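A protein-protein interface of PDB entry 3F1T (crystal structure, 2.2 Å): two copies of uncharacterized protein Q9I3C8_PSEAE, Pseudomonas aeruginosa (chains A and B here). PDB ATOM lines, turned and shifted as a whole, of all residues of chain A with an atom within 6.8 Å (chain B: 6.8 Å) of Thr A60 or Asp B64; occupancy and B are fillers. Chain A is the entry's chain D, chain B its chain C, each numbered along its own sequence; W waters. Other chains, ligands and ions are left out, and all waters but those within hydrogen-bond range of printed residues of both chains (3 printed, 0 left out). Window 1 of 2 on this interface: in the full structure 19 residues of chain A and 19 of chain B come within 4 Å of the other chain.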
ATOM      1  N   HIS A  55     -16.678 -18.221  28.622  1.00  0.00           N
ATOM      2  CA  HIS A  55     -16.557 -16.903  29.229  1.00  0.00           C
ATOM      3  C   HIS A  55     -17.180 -15.839  28.331  1.00  0.00           C
ATOM      4  O   HIS A  55     -16.900 -15.788  27.134  1.00  0.00           O
ATOM      5  CB  HIS A  55     -15.089 -16.570  29.484  1.00  0.00           C
ATOM      6  CG  HIS A  55     -14.884 -15.240  30.138  1.00  0.00           C
ATOM      7  ND1 HIS A  55     -13.985 -14.305  29.663  1.00  0.00           N
ATOM      8  CD2 HIS A  55     -15.527 -14.654  31.183  1.00  0.00           C
ATOM      9  CE1 HIS A  55     -14.053 -13.217  30.411  1.00  0.00           C
ATOM     10  NE2 HIS A  55     -14.987 -13.400  31.336  1.00  0.00           N
ATOM     11  N   GLY A  56     -18.026 -14.992  28.909  1.00  0.00           N
ATOM     12  CA  GLY A  56     -18.596 -13.876  28.172  1.00  0.00           C
ATOM     13  C   GLY A  56     -17.528 -13.124  27.408  1.00  0.00           C
ATOM     14  O   GLY A  56     -17.703 -12.800  26.236  1.00  0.00           O
ATOM     15  N   GLY A  57     -16.369 -12.951  28.035  1.00  0.00           N
ATOM     16  CA  GLY A  57     -15.317 -12.119  27.461  1.00  0.00           C
ATOM     17  C   GLY A  57     -14.835 -12.615  26.114  1.00  0.00           C
ATOM     18  O   GLY A  57     -14.440 -11.818  25.245  1.00  0.00           O
ATOM     19  N   ALA A  58     -14.801 -13.935  25.953  1.00  0.00           N
ATOM     20  CA  ALA A  58     -14.290 -14.557  24.721  1.00  0.00           C
ATOM     21  C   ALA A  58     -15.282 -14.356  23.581  1.00  0.00           C
ATOM     22  O   ALA A  58     -14.890 -14.067  22.440  1.00  0.00           O
ATOM     23  CB  ALA A  58     -14.026 -16.040  24.943  1.00  0.00           C
ATOM     24  N   ILE A  59     -16.560 -14.298  23.950  1.00  0.00           N
ATOM     25  CA  ILE A  59     -17.647 -14.013  23.019  1.00  0.00           C
ATOM     26  C   ILE A  59     -17.725 -12.536  22.624  1.00  0.00           C
ATOM     27  O   ILE A  59     -17.905 -12.224  21.453  1.00  0.00           O
ATOM     28  CB  ILE A  59     -18.984 -14.516  23.584  1.00  0.00           C
ATOM     29  CG1 ILE A  59     -18.953 -16.045  23.689  1.00  0.00           C
ATOM     30  CG2 ILE A  59     -20.143 -14.112  22.708  1.00  0.00           C
ATOM     31  CD1 ILE A  59     -20.118 -16.605  24.395  1.00  0.00           C
ATOM     32  N   THR A  60     -17.361 -11.650  23.553  1.00  0.00           N
ATOM     33  CA  THR A  60     -17.234 -10.229  23.248  1.00  0.00           C
ATOM     34  C   THR A  60     -16.140 -10.010  22.221  1.00  0.00           C
ATOM     35  O   THR A  60     -16.279  -9.174  21.317  1.00  0.00           O
ATOM     36  CB  THR A  60     -16.872  -9.395  24.506  1.00  0.00           C
ATOM     37  OG1 THR A  60     -17.916  -9.500  25.478  1.00  0.00           O
ATOM     38  CG2 THR A  60     -16.697  -7.942  24.141  1.00  0.00           C
ATOM     39  N   THR A  61     -15.006 -10.680  22.415  1.00  0.00           N
ATOM     40  CA  THR A  61     -13.924 -10.599  21.445  1.00  0.00           C
ATOM     41  C   THR A  61     -14.381 -11.132  20.106  1.00  0.00           C
ATOM     42  O   THR A  61     -14.155 -10.509  19.066  1.00  0.00           O
ATOM     43  CB  THR A  61     -12.670 -11.354  21.913  1.00  0.00           C
ATOM     44  OG1 THR A  61     -12.299 -10.872  23.208  1.00  0.00           O
ATOM     45  CG2 THR A  61     -11.508 -11.084  20.965  1.00  0.00           C
ATOM     46  N   LEU A  62     -14.969 -12.318  20.128  1.00  0.00           N
ATOM     47  CA  LEU A  62     -15.572 -12.887  18.935  1.00  0.00           C
ATOM     48  C   LEU A  62     -16.444 -11.899  18.165  1.00  0.00           C
ATOM     49  O   LEU A  62     -16.273 -11.734  16.966  1.00  0.00           O
ATOM     50  CB  LEU A  62     -16.377 -14.143  19.278  1.00  0.00           C
ATOM     51  CG  LEU A  62     -17.240 -14.712  18.139  1.00  0.00           C
ATOM     52  CD1 LEU A  62     -16.362 -15.191  16.979  1.00  0.00           C
ATOM     53  CD2 LEU A  62     -18.124 -15.825  18.670  1.00  0.00           C
ATOM     54  N   MET A  63     -17.426 -11.302  18.838  1.00  0.00           N
ATOM     55  CA  MET A  63     -18.363 -10.415  18.153  1.00  0.00           C
ATOM     56  C   MET A  63     -17.730  -9.098  17.714  1.00  0.00           C
ATOM     57  O   MET A  63     -17.823  -8.715  16.531  1.00  0.00           O
ATOM     58  CB  MET A  63     -19.608 -10.171  19.003  1.00  0.00           C
ATOM     59  CG  MET A  63     -20.513 -11.395  19.124  1.00  0.00           C
ATOM     60  SD  MET A  63     -20.679 -12.425  17.460  1.00  0.00           S
ATOM     61  CE  MET A  63     -21.218 -10.960  16.224  1.00  0.00           C
ATOM     62  N   ASP A  64     -16.988  -8.461  18.619  1.00  0.00           N
ATOM     63  CA  ASP A  64     -16.251  -7.249  18.244  1.00  0.00           C
ATOM     64  C   ASP A  64     -15.359  -7.474  17.029  1.00  0.00           C
ATOM     65  O   ASP A  64     -15.417  -6.715  16.053  1.00  0.00           O
ATOM     66  CB  ASP A  64     -15.429  -6.682  19.412  1.00  0.00           C
ATOM     67  CG  ASP A  64     -14.706  -5.380  19.038  1.00  0.00           C
ATOM     68  OD1 ASP A  64     -15.285  -4.549  18.293  1.00  0.00           O
ATOM     69  OD2 ASP A  64     -13.494  -5.273  19.324  1.00  0.00           O
ATOM     70  N   THR A  65     -14.660  -8.604  17.015  1.00  0.00           N
ATOM     71  CA  THR A  65     -13.817  -8.958  15.874  1.00  0.00           C
ATOM     72  C   THR A  65     -14.615  -9.291  14.608  1.00  0.00           C
ATOM     73  O   THR A  65     -14.213  -8.949  13.499  1.00  0.00           O
ATOM     74  CB  THR A  65     -12.893 -10.130  16.214  1.00  0.00           C
ATOM     75  OG1 THR A  65     -12.241  -9.874  17.465  1.00  0.00           O
ATOM     76  CG2 THR A  65     -11.862 -10.315  15.135  1.00  0.00           C
ATOM     77  N   THR A  66     -15.678 -10.070  14.762  1.00  0.00           N
ATOM     78  CA  THR A  66     -16.565 -10.340  13.643  1.00  0.00           C
ATOM     79  C   THR A  66     -17.157  -9.070  13.043  1.00  0.00           C
ATOM     80  O   THR A  66     -17.171  -8.907  11.821  1.00  0.00           O
ATOM     81  CB  THR A  66     -17.679 -11.313  14.041  1.00  0.00           C
ATOM     82  OG1 THR A  66     -17.093 -12.492  14.606  1.00  0.00           O
ATOM     83  CG2 THR A  66     -18.494 -11.710  12.824  1.00  0.00           C
ATOM     84  N   LEU A  86     -20.132  -0.301  20.442  1.00  0.00           N
ATOM     85  CA  LEU A  86     -20.544  -1.699  20.370  1.00  0.00           C
ATOM     86  C   LEU A  86     -21.671  -1.949  21.366  1.00  0.00           C
ATOM     87  O   LEU A  86     -21.710  -1.324  22.430  1.00  0.00           O
ATOM     88  CB  LEU A  86     -19.348  -2.605  20.675  1.00  0.00           C
ATOM     89  CG  LEU A  86     -19.408  -4.047  20.169  1.00  0.00           C
ATOM     90  CD1 LEU A  86     -19.287  -4.091  18.655  1.00  0.00           C
ATOM     91  CD2 LEU A  86     -18.281  -4.842  20.814  1.00  0.00           C
ATOM     92  N   ILE A  88     -23.841  -5.421  22.923  1.00  0.00           N
ATOM     93  CA  ILE A  88     -24.062  -6.850  22.939  1.00  0.00           C
ATOM     94  C   ILE A  88     -25.148  -7.151  23.955  1.00  0.00           C
ATOM     95  O   ILE A  88     -25.060  -6.710  25.096  1.00  0.00           O
ATOM     96  CB  ILE A  88     -22.768  -7.585  23.354  1.00  0.00           C
ATOM     97  CG1 ILE A  88     -21.583  -7.063  22.530  1.00  0.00           C
ATOM     98  CG2 ILE A  88     -22.940  -9.083  23.220  1.00  0.00           C
ATOM     99  CD1 ILE A  88     -20.299  -7.849  22.708  1.00  0.00           C
ATOM    100  N   TYR A  90     -27.051 -10.575  25.468  1.00  0.00           N
ATOM    101  CA  TYR A  90     -27.282 -12.014  25.594  1.00  0.00           C
ATOM    102  C   TYR A  90     -28.745 -12.380  25.725  1.00  0.00           C
ATOM    103  O   TYR A  90     -29.464 -11.805  26.550  1.00  0.00           O
ATOM    104  CB  TYR A  90     -26.517 -12.552  26.781  1.00  0.00           C
ATOM    105  CG  TYR A  90     -25.042 -12.586  26.533  1.00  0.00           C
ATOM    106  CD1 TYR A  90     -24.447 -13.706  25.954  1.00  0.00           C
ATOM    107  CD2 TYR A  90     -24.277 -11.433  26.670  1.00  0.00           C
ATOM    108  CE1 TYR A  90     -23.109 -13.714  25.649  1.00  0.00           C
ATOM    109  CE2 TYR A  90     -22.933 -11.436  26.388  1.00  0.00           C
ATOM    110  CZ  TYR A  90     -22.354 -12.574  25.864  1.00  0.00           C
ATOM    111  OH  TYR A  90     -21.015 -12.577  25.564  1.00  0.00           O
ATOM    112  N   ILE B  59      -8.550  -2.703  24.497  1.00  0.00           N
ATOM    113  CA  ILE B  59      -9.250  -1.786  25.377  1.00  0.00           C
ATOM    114  C   ILE B  59     -10.691  -2.238  25.629  1.00  0.00           C
ATOM    115  O   ILE B  59     -11.190  -2.193  26.762  1.00  0.00           O
ATOM    116  CB  ILE B  59      -9.218  -0.346  24.795  1.00  0.00           C
ATOM    117  CG1 ILE B  59      -7.767   0.083  24.556  1.00  0.00           C
ATOM    118  CG2 ILE B  59      -9.942   0.623  25.713  1.00  0.00           C
ATOM    119  CD1 ILE B  59      -7.615   1.498  24.005  1.00  0.00           C
ATOM    120  N   THR B  60     -11.316  -2.802  24.603  1.00  0.00           N
ATOM    121  CA  THR B  60     -12.656  -3.345  24.766  1.00  0.00           C
ATOM    122  C   THR B  60     -12.649  -4.532  25.721  1.00  0.00           C
ATOM    123  O   THR B  60     -13.441  -4.588  26.666  1.00  0.00           O
ATOM    124  CB  THR B  60     -13.279  -3.696  23.399  1.00  0.00           C
ATOM    125  OG1 THR B  60     -13.513  -2.477  22.672  1.00  0.00           O
ATOM    126  CG2 THR B  60     -14.603  -4.442  23.570  1.00  0.00           C
ATOM    127  N   THR B  61     -11.644  -5.387  25.576  1.00  0.00           N
ATOM    128  CA  THR B  61     -11.429  -6.462  26.519  1.00  0.00           C
ATOM    129  C   THR B  61     -11.209  -5.870  27.911  1.00  0.00           C
ATOM    130  O   THR B  61     -11.728  -6.378  28.887  1.00  0.00           O
ATOM    131  CB  THR B  61     -10.193  -7.299  26.133  1.00  0.00           C
ATOM    132  OG1 THR B  61     -10.410  -7.918  24.857  1.00  0.00           O
ATOM    133  CG2 THR B  61      -9.953  -8.383  27.162  1.00  0.00           C
ATOM    134  N   LEU B  62     -10.374  -4.837  27.999  1.00  0.00           N
ATOM    135  CA  LEU B  62     -10.051  -4.232  29.298  1.00  0.00           C
ATOM    136  C   LEU B  62     -11.326  -3.789  29.994  1.00  0.00           C
ATOM    137  O   LEU B  62     -11.498  -3.991  31.205  1.00  0.00           O
ATOM    138  CB  LEU B  62      -9.127  -3.027  29.111  1.00  0.00           C
ATOM    139  CG  LEU B  62      -9.029  -2.065  30.296  1.00  0.00           C
ATOM    140  CD1 LEU B  62      -8.261  -2.733  31.426  1.00  0.00           C
ATOM    141  CD2 LEU B  62      -8.382  -0.742  29.875  1.00  0.00           C
ATOM    142  N   MET B  63     -12.201  -3.133  29.241  1.00  0.00           N
ATOM    143  CA  MET B  63     -13.389  -2.530  29.832  1.00  0.00           C
ATOM    144  C   MET B  63     -14.402  -3.608  30.212  1.00  0.00           C
ATOM    145  O   MET B  63     -14.936  -3.621  31.325  1.00  0.00           O
ATOM    146  CB  MET B  63     -14.008  -1.538  28.850  1.00  0.00           C
ATOM    147  CG  MET B  63     -13.191  -0.275  28.669  1.00  0.00           C
ATOM    148  SD  MET B  63     -14.225   1.133  27.830  1.00  0.00           S
ATOM    149  CE  MET B  63     -14.350   0.356  26.049  1.00  0.00           C
ATOM    150  N   ASP B  64     -14.547  -4.589  29.330  1.00  0.00           N
ATOM    151  CA  ASP B  64     -15.403  -5.730  29.597  1.00  0.00           C
ATOM    152  C   ASP B  64     -14.939  -6.467  30.842  1.00  0.00           C
ATOM    153  O   ASP B  64     -15.755  -6.848  31.669  1.00  0.00           O
ATOM    154  CB  ASP B  64     -15.386  -6.674  28.398  1.00  0.00           C
ATOM    155  CG  ASP B  64     -16.358  -7.840  28.551  1.00  0.00           C
ATOM    156  OD1 ASP B  64     -17.147  -7.859  29.524  1.00  0.00           O
ATOM    157  OD2 ASP B  64     -16.278  -8.782  27.746  1.00  0.00           O
ATOM    158  N   THR B  65     -13.641  -6.773  30.911  1.00  0.00           N
ATOM    159  CA  THR B  65     -13.072  -7.464  32.071  1.00  0.00           C
ATOM    160  C   THR B  65     -13.250  -6.650  33.360  1.00  0.00           C
ATOM    161  O   THR B  65     -13.584  -7.206  34.403  1.00  0.00           O
ATOM    162  CB  THR B  65     -11.587  -7.766  31.852  1.00  0.00           C
ATOM    163  OG1 THR B  65     -11.417  -8.402  30.583  1.00  0.00           O
ATOM    164  CG2 THR B  65     -11.042  -8.672  32.951  1.00  0.00           C
ATOM    165  N   THR B  66     -13.068  -5.331  33.282  1.00  0.00           N
ATOM    166  CA  THR B  66     -13.200  -4.467  34.451  1.00  0.00           C
ATOM    167  C   THR B  66     -14.631  -4.472  34.988  1.00  0.00           C
ATOM    168  O   THR B  66     -14.853  -4.477  36.210  1.00  0.00           O
ATOM    169  CB  THR B  66     -12.760  -3.004  34.143  1.00  0.00           C
ATOM    170  OG1 THR B  66     -11.460  -3.015  33.530  1.00  0.00           O
ATOM    171  CG2 THR B  66     -12.696  -2.183  35.411  1.00  0.00           C
ATOM    172  N   CYS B  67     -15.602  -4.359  34.082  1.00  0.00           N
ATOM    173  CA  CYS B  67     -17.014  -4.462  34.458  1.00  0.00           C
ATOM    174  C   CYS B  67     -17.351  -5.819  35.058  1.00  0.00           C
ATOM    175  O   CYS B  67     -17.945  -5.895  36.120  1.00  0.00           O
ATOM    176  CB  CYS B  67     -17.908  -4.195  33.257  1.00  0.00           C
ATOM    177  SG  CYS B  67     -17.988  -2.466  32.845  1.00  0.00           S
ATOM    178  N   GLY B  68     -16.954  -6.886  34.373  1.00  0.00           N
ATOM    179  CA  GLY B  68     -17.216  -8.239  34.854  1.00  0.00           C
ATOM    180  C   GLY B  68     -16.644  -8.555  36.224  1.00  0.00           C
ATOM    181  O   GLY B  68     -17.182  -9.401  36.956  1.00  0.00           O
ATOM    182  N   ILE B  69     -15.520  -7.932  36.560  1.00  0.00           N
ATOM    183  CA  ILE B  69     -14.836  -8.255  37.809  1.00  0.00           C
ATOM    184  C   ILE B  69     -15.215  -7.261  38.896  1.00  0.00           C
ATOM    185  O   ILE B  69     -15.078  -7.552  40.078  1.00  0.00           O
ATOM    186  CB  ILE B  69     -13.302  -8.271  37.637  1.00  0.00           C
ATOM    187  CG1 ILE B  69     -12.887  -9.373  36.677  1.00  0.00           C
ATOM    188  CG2 ILE B  69     -12.613  -8.493  38.981  1.00  0.00           C
ATOM    189  CD1 ILE B  69     -11.395  -9.392  36.397  1.00  0.00           C
ATOM    190  N   THR B  83     -22.350 -12.406  31.600  1.00  0.00           N
ATOM    191  CA  THR B  83     -22.761 -11.151  30.975  1.00  0.00           C
ATOM    192  C   THR B  83     -24.219 -11.197  30.511  1.00  0.00           C
ATOM    193  O   THR B  83     -24.622 -12.107  29.788  1.00  0.00           O
ATOM    194  CB  THR B  83     -21.855 -10.803  29.782  1.00  0.00           C
ATOM    195  OG1 THR B  83     -20.483 -10.883  30.192  1.00  0.00           O
ATOM    196  CG2 THR B  83     -22.145  -9.387  29.276  1.00  0.00           C
ATOM    197  N   LEU B  86     -23.747  -5.458  27.410  1.00  0.00           N
ATOM    198  CA  LEU B  86     -22.584  -4.580  27.419  1.00  0.00           C
ATOM    199  C   LEU B  86     -22.863  -3.424  26.474  1.00  0.00           C
ATOM    200  O   LEU B  86     -23.503  -3.617  25.443  1.00  0.00           O
ATOM    201  CB  LEU B  86     -21.361  -5.344  26.909  1.00  0.00           C
ATOM    202  CG  LEU B  86     -20.195  -5.685  27.854  1.00  0.00           C
ATOM    203  CD1 LEU B  86     -18.943  -5.919  27.016  1.00  0.00           C
ATOM    204  CD2 LEU B  86     -19.944  -4.604  28.892  1.00  0.00           C
ATOM    205  N   ILE B  88     -20.504  -0.292  24.958  1.00  0.00           N
ATOM    206  CA  ILE B  88     -19.199   0.370  24.876  1.00  0.00           C
ATOM    207  C   ILE B  88     -19.210   1.491  23.833  1.00  0.00           C
ATOM    208  O   ILE B  88     -19.581   1.271  22.676  1.00  0.00           O
ATOM    209  CB  ILE B  88     -18.097  -0.640  24.529  1.00  0.00           C
ATOM    210  CG1 ILE B  88     -17.839  -1.550  25.734  1.00  0.00           C
ATOM    211  CG2 ILE B  88     -16.834   0.082  24.102  1.00  0.00           C
ATOM    212  CD1 ILE B  88     -16.688  -2.481  25.556  1.00  0.00           C
ATOM    213  N   VAL B 132     -18.273   2.587  29.227  1.00  0.00           N
ATOM    214  CA  VAL B 132     -18.852   1.245  29.153  1.00  0.00           C
ATOM    215  C   VAL B 132     -19.933   1.055  30.238  1.00  0.00           C
ATOM    216  O   VAL B 132     -19.792   1.542  31.368  1.00  0.00           O
ATOM    217  CB  VAL B 132     -17.754   0.173  29.323  1.00  0.00           C
ATOM    218  CG1 VAL B 132     -17.037   0.377  30.646  1.00  0.00           C
ATOM    219  CG2 VAL B 132     -18.323  -1.246  29.215  1.00  0.00           C
ATOM    220  N   PHE B 136     -24.807  -7.879  34.783  1.00  0.00           N
ATOM    221  CA  PHE B 136     -24.307  -9.238  34.940  1.00  0.00           C
ATOM    222  C   PHE B 136     -25.209 -10.054  35.858  1.00  0.00           C
ATOM    223  O   PHE B 136     -25.877  -9.506  36.721  1.00  0.00           O
ATOM    224  CB  PHE B 136     -22.875  -9.214  35.485  1.00  0.00           C
ATOM    225  CG  PHE B 136     -21.894  -8.502  34.590  1.00  0.00           C
ATOM    226  CD1 PHE B 136     -21.749  -7.124  34.649  1.00  0.00           C
ATOM    227  CD2 PHE B 136     -21.090  -9.215  33.722  1.00  0.00           C
ATOM    228  CE1 PHE B 136     -20.822  -6.469  33.845  1.00  0.00           C
ATOM    229  CE2 PHE B 136     -20.181  -8.567  32.899  1.00  0.00           C
ATOM    230  CZ  PHE B 136     -20.079  -7.187  32.935  1.00  0.00           C
HETATM  231  O   HOH W   1     -12.986  -2.880  20.177  1.00  0.00           O
HETATM  232  O   HOH W   2     -18.439 -10.231  28.510  1.00  0.00           O
HETATM  233  O   HOH W   3     -21.164 -14.261  29.896  1.00  0.00           O
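The side-chain carboxylate (OD2) of Asp B64 is in hydrogen-bond range of the side-chain hydroxyl (OG1) of Thr A60, at 2.9 Å.
O of Ile A88 lies within hydrogen-bond range of N of Leu B86.
The backbone carbonyl oxygen (O) of Ile B88 lies within hydrogen-bond range of the backbone NH (N) of Leu A86.
OG1 of Thr A60 lies within hydrogen-bond range of O of Gly A56 (3.4 Å).
O of Thr B61 is in hydrogen-bond range of OG1 of Thr B65 (2.7 Å).
A ring nitrogen (ND1) of His A55 lies close to the backbone NH (N) of Gly A57, 3.2 Å away.
The side-chain hydroxyl of Thr A61 sits at hydrogen-bond distance from the backbone carbonyl oxygen of Gly A57 (3.1 Å).
O of Gly A56 lies within hydrogen-bond range of OH of Tyr A90 (3.4 Å).
The backbone carbonyl oxygen (O) of Thr A61 is in hydrogen-bond range of the side-chain hydroxyl (OG1) of Thr A65 (2.6 Å).
Gly A57 touches Asp B64.
OG1 of Thr B61 touches OG1 of Thr A61, 3.9 Å away.
Thr B83 touches Tyr A90.
Printed residues of chain B within 4 Å of Gly A57: Asp B64.
Thr A60 touches just one residue of chain B: Asp B64.
Of the printed residues of chain B, Thr A61 touches Thr B61.
Ile B59 touches none of the printed residues of chain A.
Asp B64 touches two residues of chain A.
The nearest residue of chain B that does not touch Thr A60 is Leu B86 (4.03 Å).
The nearest printed residue of chain B that does not touch Tyr A90 is Leu B86 (6.0 Å).
Of the 16 printed residues of chain B, 5 touch a printed residue of chain A.
Of the 15 printed residues of chain A, 6 touch a printed residue of chain B.
Among the printed residues, 6 pairs touch across the chains.
Among the printed residues, no Asp or Glu carboxylate lies within 4 Å of a Lys or Arg side-chain nitrogen of the other chain.
Thr A60 touches Asp B64, but with the chains exchanged Asp A64 does not touch Thr B60 (4.4 Å).
Thr A61 touches its own counterpart, Thr B61.
Leu A86 touches Ile B88, and with the chains exchanged Ile A88 touches Leu B86.
Positions printed for both chains: 59, 60, 61, 62, 63, 64, 65, 66, 86 and 88.
Water W1 bridges OG1 of Thr B60 and OD2 of Asp A64.
Water W2 lies within hydrogen-bond range of OD2 of Asp B64, OG1 of Thr B83, OG1 of Thr A60 and N of Gly A57.
Water W3 bridges N of Thr B83 (2.8 Å) and N of Gly A56 (3.4 Å).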
